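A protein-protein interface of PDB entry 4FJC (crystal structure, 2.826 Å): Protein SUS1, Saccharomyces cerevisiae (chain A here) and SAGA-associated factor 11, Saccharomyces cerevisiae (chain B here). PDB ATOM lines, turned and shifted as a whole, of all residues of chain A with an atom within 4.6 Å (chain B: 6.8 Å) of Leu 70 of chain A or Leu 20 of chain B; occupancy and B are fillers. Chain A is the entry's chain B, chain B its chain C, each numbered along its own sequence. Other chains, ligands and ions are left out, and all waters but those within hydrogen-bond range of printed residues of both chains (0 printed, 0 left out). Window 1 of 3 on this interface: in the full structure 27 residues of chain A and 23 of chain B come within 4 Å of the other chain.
The side-chain carboxylate (OE2) of Glu 66 of chain A lies close to the side-chain amide oxygen (OE1) of Gln 25 of chain B.
O of Thr 21 of chain B sits close to OE1 of Gln 25 of chain B, 3.3 Å away.
The backbone carbonyl oxygen (O) of Asn 18 of chain B lies within hydrogen-bond range of the side-chain hydroxyl (OG1) of Thr 21 of chain B.
The backbone carbonyl oxygen of Val 73 of chain A sits at hydrogen-bond distance from the guanidinium group of Arg 78 of chain A, at 2.8 Å.
The guanidinium group (NH2) of Arg 78 of chain A sits at hydrogen-bond distance from the backbone carbonyl oxygen (O) of Glu 71 of chain A (3.3 Å).
O of Asn 17 of chain B sits at hydrogen-bond distance from OG1 of Thr 21 of chain B, at 2.6 Å.
Leu 29 of chain A touches Leu 16 of chain B.
CD2 of Leu 29 of chain A touches CB of Leu 19 of chain B (3.6 Å).
Leu 33 of chain A touches Leu 20 of chain B (CD1 to CD2, 3.8 Å).
Leu 33 of chain A touches Leu 23 of chain B.
Thr 21 of chain B touches Glu 66 of chain A.
Ile 24 of chain B touches Ala 69 of chain A (CD1 to CB, 3.4 Å).
Leu 70 of chain A touches Leu 20 of chain B.
Leu 70 of chain A touches Ile 24 of chain B (CD2 to CD1, 3.8 Å).
Arg 78 of chain A touches Leu 16 of chain B (CG to CD2, 3.9 Å).
Of chain B, only Leu 20 (3.8 Å) and Ile 24 (3.8 Å) come within 4 Å of Leu 70 of chain A.
Printed residues of chain A within 4 Å of Leu 20 of chain B: Leu 33 (3.8 Å) and Leu 70 (3.8 Å).
Of the printed residues of chain A, Thr 21 of chain B touches Glu 66.
Of the printed residues of chain B, Glu 66 of chain A touches Thr 21 and Gln 25.
Of the printed residues of chain A, Leu 16 of chain B touches Leu 29 and Arg 78.
Of the printed residues of chain B, Leu 29 of chain A touches Leu 16 and Leu 19.
The nearest residue of chain B that does not touch Leu 70 of chain A is Asn 17 of chain B (4.2 Å).
Of the 11 printed residues of chain B, 7 touch a printed residue of chain A.
Hydrophobic or aromatic side chains of chain B within 4 Å of the printed part of chain A: Leu 16, Leu 19, Leu 20, Leu 23 and Ile 24.
Printed residues of chain A that touch a printed residue of chain B: Leu 29, Leu 33, Glu 66, Ala 69, Leu 70 and Arg 78.
Among the printed residues, 10 pairs touch across the chains.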
ATOM      1  N   LEU A  29       5.161  11.225  29.127  1.00  0.00           N
ATOM      2  CA  LEU A  29       4.788  12.625  29.268  1.00  0.00           C
ATOM      3  C   LEU A  29       3.300  12.796  28.967  1.00  0.00           C
ATOM      4  O   LEU A  29       2.583  13.362  29.768  1.00  0.00           O
ATOM      5  CB  LEU A  29       5.676  13.494  28.380  1.00  0.00           C
ATOM      6  CG  LEU A  29       5.443  15.008  28.334  1.00  0.00           C
ATOM      7  CD1 LEU A  29       5.395  15.643  29.720  1.00  0.00           C
ATOM      8  CD2 LEU A  29       6.497  15.674  27.442  1.00  0.00           C
ATOM      9  N   LEU A  33       0.188  14.087  31.363  1.00  0.00           N
ATOM     10  CA  LEU A  33      -0.499  15.341  31.076  1.00  0.00           C
ATOM     11  C   LEU A  33      -1.958  15.078  30.762  1.00  0.00           C
ATOM     12  O   LEU A  33      -2.828  15.812  31.232  1.00  0.00           O
ATOM     13  CB  LEU A  33       0.180  16.082  29.929  1.00  0.00           C
ATOM     14  CG  LEU A  33       1.544  16.739  30.211  1.00  0.00           C
ATOM     15  CD1 LEU A  33       2.120  17.306  28.918  1.00  0.00           C
ATOM     16  CD2 LEU A  33       1.445  17.823  31.277  1.00  0.00           C
ATOM     17  N   GLU A  66       0.733  29.241  24.101  1.00  0.00           N
ATOM     18  CA  GLU A  66       1.920  28.458  24.443  1.00  0.00           C
ATOM     19  C   GLU A  66       2.522  28.819  25.798  1.00  0.00           C
ATOM     20  O   GLU A  66       2.864  27.912  26.567  1.00  0.00           O
ATOM     21  CB  GLU A  66       3.023  28.508  23.351  1.00  0.00           C
ATOM     22  CG  GLU A  66       3.954  27.301  23.430  1.00  0.00           C
ATOM     23  CD  GLU A  66       4.920  27.145  22.255  1.00  0.00           C
ATOM     24  OE1 GLU A  66       5.749  28.048  21.982  1.00  0.00           O
ATOM     25  OE2 GLU A  66       4.900  26.072  21.608  1.00  0.00           O
ATOM     26  N   PRO A  67       2.678  30.122  26.101  1.00  0.00           N
ATOM     27  CA  PRO A  67       3.430  30.355  27.315  1.00  0.00           C
ATOM     28  C   PRO A  67       2.595  29.992  28.553  1.00  0.00           C
ATOM     29  O   PRO A  67       3.150  29.442  29.513  1.00  0.00           O
ATOM     30  CB  PRO A  67       3.785  31.855  27.241  1.00  0.00           C
ATOM     31  CG  PRO A  67       3.522  32.262  25.829  1.00  0.00           C
ATOM     32  CD  PRO A  67       2.390  31.381  25.396  1.00  0.00           C
ATOM     33  N   LYS A  68       1.289  30.273  28.549  1.00  0.00           N
ATOM     34  CA  LYS A  68       0.435  29.804  29.642  1.00  0.00           C
ATOM     35  C   LYS A  68       0.462  28.257  29.682  1.00  0.00           C
ATOM     36  O   LYS A  68       0.589  27.657  30.745  1.00  0.00           O
ATOM     37  CB  LYS A  68      -1.004  30.322  29.485  1.00  0.00           C
ATOM     38  CG  LYS A  68      -1.165  31.840  29.661  1.00  0.00           C
ATOM     39  CD  LYS A  68      -2.581  32.404  29.353  1.00  0.00           C
ATOM     40  CE  LYS A  68      -2.877  33.740  30.063  1.00  0.00           C
ATOM     41  NZ  LYS A  68      -4.313  33.936  30.465  1.00  0.00           N
ATOM     42  N   ALA A  69       0.349  27.616  28.515  1.00  0.00           N
ATOM     43  CA  ALA A  69       0.295  26.164  28.444  1.00  0.00           C
ATOM     44  C   ALA A  69       1.461  25.554  29.190  1.00  0.00           C
ATOM     45  O   ALA A  69       1.291  24.633  29.995  1.00  0.00           O
ATOM     46  CB  ALA A  69       0.304  25.693  26.997  1.00  0.00           C
ATOM     47  N   LEU A  70       2.648  26.089  28.917  1.00  0.00           N
ATOM     48  CA  LEU A  70       3.869  25.634  29.551  1.00  0.00           C
ATOM     49  C   LEU A  70       3.819  25.737  31.058  1.00  0.00           C
ATOM     50  O   LEU A  70       4.158  24.772  31.712  1.00  0.00           O
ATOM     51  CB  LEU A  70       5.069  26.401  29.027  1.00  0.00           C
ATOM     52  CG  LEU A  70       5.550  26.032  27.626  1.00  0.00           C
ATOM     53  CD1 LEU A  70       6.664  26.986  27.225  1.00  0.00           C
ATOM     54  CD2 LEU A  70       6.010  24.569  27.586  1.00  0.00           C
ATOM     55  N   GLU A  71       3.389  26.870  31.619  1.00  0.00           N
ATOM     56  CA  GLU A  71       3.321  27.016  33.111  1.00  0.00           C
ATOM     57  C   GLU A  71       2.446  25.952  33.776  1.00  0.00           C
ATOM     58  O   GLU A  71       2.831  25.381  34.783  1.00  0.00           O
ATOM     59  CB  GLU A  71       2.858  28.417  33.565  1.00  0.00           C
ATOM     60  CG  GLU A  71       3.995  29.331  34.015  1.00  0.00           C
ATOM     61  CD  GLU A  71       3.518  30.690  34.563  1.00  0.00           C
ATOM     62  OE1 GLU A  71       4.295  31.342  35.322  1.00  0.00           O
ATOM     63  OE2 GLU A  71       2.371  31.118  34.242  1.00  0.00           O
ATOM     64  N   MET A  72       1.304  25.662  33.158  1.00  0.00           N
ATOM     65  CA  MET A  72       0.288  24.726  33.690  1.00  0.00           C
ATOM     66  C   MET A  72       0.800  23.307  33.994  1.00  0.00           C
ATOM     67  O   MET A  72       0.181  22.578  34.749  1.00  0.00           O
ATOM     68  CB  MET A  72      -0.894  24.621  32.706  1.00  0.00           C
ATOM     69  CG  MET A  72      -1.580  25.944  32.382  1.00  0.00           C
ATOM     70  SD  MET A  72      -3.009  25.742  31.296  1.00  0.00           S
ATOM     71  CE  MET A  72      -4.038  27.117  31.832  1.00  0.00           C
ATOM     72  N   VAL A  73       1.915  22.904  33.413  1.00  0.00           N
ATOM     73  CA  VAL A  73       2.340  21.532  33.587  1.00  0.00           C
ATOM     74  C   VAL A  73       2.773  21.409  35.058  1.00  0.00           C
ATOM     75  O   VAL A  73       3.472  22.278  35.570  1.00  0.00           O
ATOM     76  CB  VAL A  73       3.388  21.067  32.506  1.00  0.00           C
ATOM     77  CG1 VAL A  73       3.362  21.969  31.275  1.00  0.00           C
ATOM     78  CG2 VAL A  73       4.798  20.966  33.054  1.00  0.00           C
ATOM     79  N   ARG A  78       6.539  17.671  35.528  1.00  0.00           N
ATOM     80  CA  ARG A  78       7.785  18.287  35.123  1.00  0.00           C
ATOM     81  C   ARG A  78       8.983  17.600  35.826  1.00  0.00           C
ATOM     82  O   ARG A  78       9.908  17.162  35.149  1.00  0.00           O
ATOM     83  CB  ARG A  78       7.740  19.790  35.397  1.00  0.00           C
ATOM     84  CG  ARG A  78       8.822  20.585  34.686  1.00  0.00           C
ATOM     85  CD  ARG A  78       8.946  21.992  35.242  1.00  0.00           C
ATOM     86  NE  ARG A  78       7.638  22.634  35.412  1.00  0.00           N
ATOM     87  CZ  ARG A  78       6.916  23.193  34.430  1.00  0.00           C
ATOM     88  NH1 ARG A  78       7.356  23.201  33.154  1.00  0.00           N
ATOM     89  NH2 ARG A  78       5.731  23.753  34.728  1.00  0.00           N
ATOM     90  N   ILE B  15      15.223  18.986  26.029  1.00  0.00           N
ATOM     91  CA  ILE B  15      14.475  17.882  25.493  1.00  0.00           C
ATOM     92  C   ILE B  15      13.006  17.944  25.944  1.00  0.00           C
ATOM     93  O   ILE B  15      12.082  17.638  25.159  1.00  0.00           O
ATOM     94  CB  ILE B  15      15.126  16.574  25.912  1.00  0.00           C
ATOM     95  CG1 ILE B  15      16.517  16.493  25.300  1.00  0.00           C
ATOM     96  CG2 ILE B  15      14.300  15.416  25.426  1.00  0.00           C
ATOM     97  CD1 ILE B  15      17.395  15.440  25.914  1.00  0.00           C
ATOM     98  N   LEU B  16      12.793  18.363  27.194  1.00  0.00           N
ATOM     99  CA  LEU B  16      11.427  18.519  27.724  1.00  0.00           C
ATOM    100  C   LEU B  16      10.634  19.619  27.029  1.00  0.00           C
ATOM    101  O   LEU B  16       9.428  19.472  26.828  1.00  0.00           O
ATOM    102  CB  LEU B  16      11.418  18.786  29.237  1.00  0.00           C
ATOM    103  CG  LEU B  16       9.981  18.909  29.791  1.00  0.00           C
ATOM    104  CD1 LEU B  16       9.143  17.692  29.441  1.00  0.00           C
ATOM    105  CD2 LEU B  16       9.960  19.155  31.288  1.00  0.00           C
ATOM    106  N   ASN B  17      11.309  20.717  26.685  1.00  0.00           N
ATOM    107  CA  ASN B  17      10.657  21.876  26.071  1.00  0.00           C
ATOM    108  C   ASN B  17      10.251  21.606  24.617  1.00  0.00           C
ATOM    109  O   ASN B  17       9.153  21.890  24.168  1.00  0.00           O
ATOM    110  CB  ASN B  17      11.611  23.030  26.128  1.00  0.00           C
ATOM    111  CG  ASN B  17      11.028  24.272  25.558  1.00  0.00           C
ATOM    112  OD1 ASN B  17      10.143  24.867  26.143  1.00  0.00           O
ATOM    113  ND2 ASN B  17      11.530  24.685  24.419  1.00  0.00           N
ATOM    114  N   ASN B  18      11.185  21.045  23.886  1.00  0.00           N
ATOM    115  CA  ASN B  18      10.902  20.421  22.627  1.00  0.00           C
ATOM    116  C   ASN B  18       9.670  19.489  22.657  1.00  0.00           C
ATOM    117  O   ASN B  18       8.820  19.552  21.759  1.00  0.00           O
ATOM    118  CB  ASN B  18      12.116  19.619  22.218  1.00  0.00           C
ATOM    119  CG  ASN B  18      13.117  20.436  21.458  1.00  0.00           C
ATOM    120  OD1 ASN B  18      13.623  19.985  20.422  1.00  0.00           O
ATOM    121  ND2 ASN B  18      13.431  21.627  21.960  1.00  0.00           N
ATOM    122  N   LEU B  19       9.584  18.615  23.658  1.00  0.00           N
ATOM    123  CA  LEU B  19       8.485  17.689  23.695  1.00  0.00           C
ATOM    124  C   LEU B  19       7.255  18.461  24.011  1.00  0.00           C
ATOM    125  O   LEU B  19       6.199  18.177  23.484  1.00  0.00           O
ATOM    126  CB  LEU B  19       8.677  16.569  24.720  1.00  0.00           C
ATOM    127  CG  LEU B  19       9.589  15.411  24.335  1.00  0.00           C
ATOM    128  CD1 LEU B  19       9.843  14.533  25.539  1.00  0.00           C
ATOM    129  CD2 LEU B  19       9.009  14.601  23.196  1.00  0.00           C
ATOM    130  N   LEU B  20       7.375  19.451  24.874  1.00  0.00           N
ATOM    131  CA  LEU B  20       6.181  20.130  25.365  1.00  0.00           C
ATOM    132  C   LEU B  20       5.608  21.114  24.345  1.00  0.00           C
ATOM    133  O   LEU B  20       4.401  21.224  24.207  1.00  0.00           O
ATOM    134  CB  LEU B  20       6.496  20.868  26.664  1.00  0.00           C
ATOM    135  CG  LEU B  20       6.554  20.074  27.972  1.00  0.00           C
ATOM    136  CD1 LEU B  20       7.016  21.040  29.071  1.00  0.00           C
ATOM    137  CD2 LEU B  20       5.213  19.424  28.290  1.00  0.00           C
ATOM    138  N   THR B  21       6.490  21.852  23.669  1.00  0.00           N
ATOM    139  CA  THR B  21       6.099  22.794  22.623  1.00  0.00           C
ATOM    140  C   THR B  21       5.490  22.063  21.399  1.00  0.00           C
ATOM    141  O   THR B  21       4.607  22.610  20.740  1.00  0.00           O
ATOM    142  CB  THR B  21       7.295  23.690  22.187  1.00  0.00           C
ATOM    143  OG1 THR B  21       8.427  22.878  21.863  1.00  0.00           O
ATOM    144  CG2 THR B  21       7.681  24.661  23.304  1.00  0.00           C
ATOM    145  N   THR B  22       5.930  20.839  21.101  1.00  0.00           N
ATOM    146  CA  THR B  22       5.333  20.101  19.995  1.00  0.00           C
ATOM    147  C   THR B  22       3.884  19.768  20.336  1.00  0.00           C
ATOM    148  O   THR B  22       2.982  19.949  19.518  1.00  0.00           O
ATOM    149  CB  THR B  22       6.083  18.796  19.643  1.00  0.00           C
ATOM    150  OG1 THR B  22       7.429  19.093  19.239  1.00  0.00           O
ATOM    151  CG2 THR B  22       5.377  18.068  18.506  1.00  0.00           C
ATOM    152  N   LEU B  23       3.657  19.306  21.551  1.00  0.00           N
ATOM    153  CA  LEU B  23       2.340  18.858  21.960  1.00  0.00           C
ATOM    154  C   LEU B  23       1.365  20.035  21.983  1.00  0.00           C
ATOM    155  O   LEU B  23       0.179  19.898  21.615  1.00  0.00           O
ATOM    156  CB  LEU B  23       2.414  18.219  23.340  1.00  0.00           C
ATOM    157  CG  LEU B  23       1.611  16.946  23.574  1.00  0.00           C
ATOM    158  CD1 LEU B  23       1.703  16.540  25.041  1.00  0.00           C
ATOM    159  CD2 LEU B  23       0.167  17.125  23.145  1.00  0.00           C
ATOM    160  N   ILE B  24       1.849  21.196  22.414  1.00  0.00           N
ATOM    161  CA  ILE B  24       0.976  22.353  22.514  1.00  0.00           C
ATOM    162  C   ILE B  24       0.601  22.750  21.091  1.00  0.00           C
ATOM    163  O   ILE B  24      -0.581  23.046  20.783  1.00  0.00           O
ATOM    164  CB  ILE B  24       1.646  23.536  23.266  1.00  0.00           C
ATOM    165  CG1 ILE B  24       1.868  23.130  24.740  1.00  0.00           C
ATOM    166  CG2 ILE B  24       0.791  24.797  23.163  1.00  0.00           C
ATOM    167  CD1 ILE B  24       2.828  23.979  25.555  1.00  0.00           C
ATOM    168  N   GLN B  25       1.605  22.731  20.218  1.00  0.00           N
ATOM    169  CA  GLN B  25       1.387  23.246  18.899  1.00  0.00           C
ATOM    170  C   GLN B  25       0.488  22.295  18.087  1.00  0.00           C
ATOM    171  O   GLN B  25      -0.169  22.724  17.143  1.00  0.00           O
ATOM    172  CB  GLN B  25       2.708  23.504  18.205  1.00  0.00           C
ATOM    173  CG  GLN B  25       3.433  24.718  18.721  1.00  0.00           C
ATOM    174  CD  GLN B  25       4.872  24.754  18.256  1.00  0.00           C
ATOM    175  OE1 GLN B  25       5.783  25.106  19.017  1.00  0.00           O
ATOM    176  NE2 GLN B  25       5.085  24.412  16.985  1.00  0.00           N
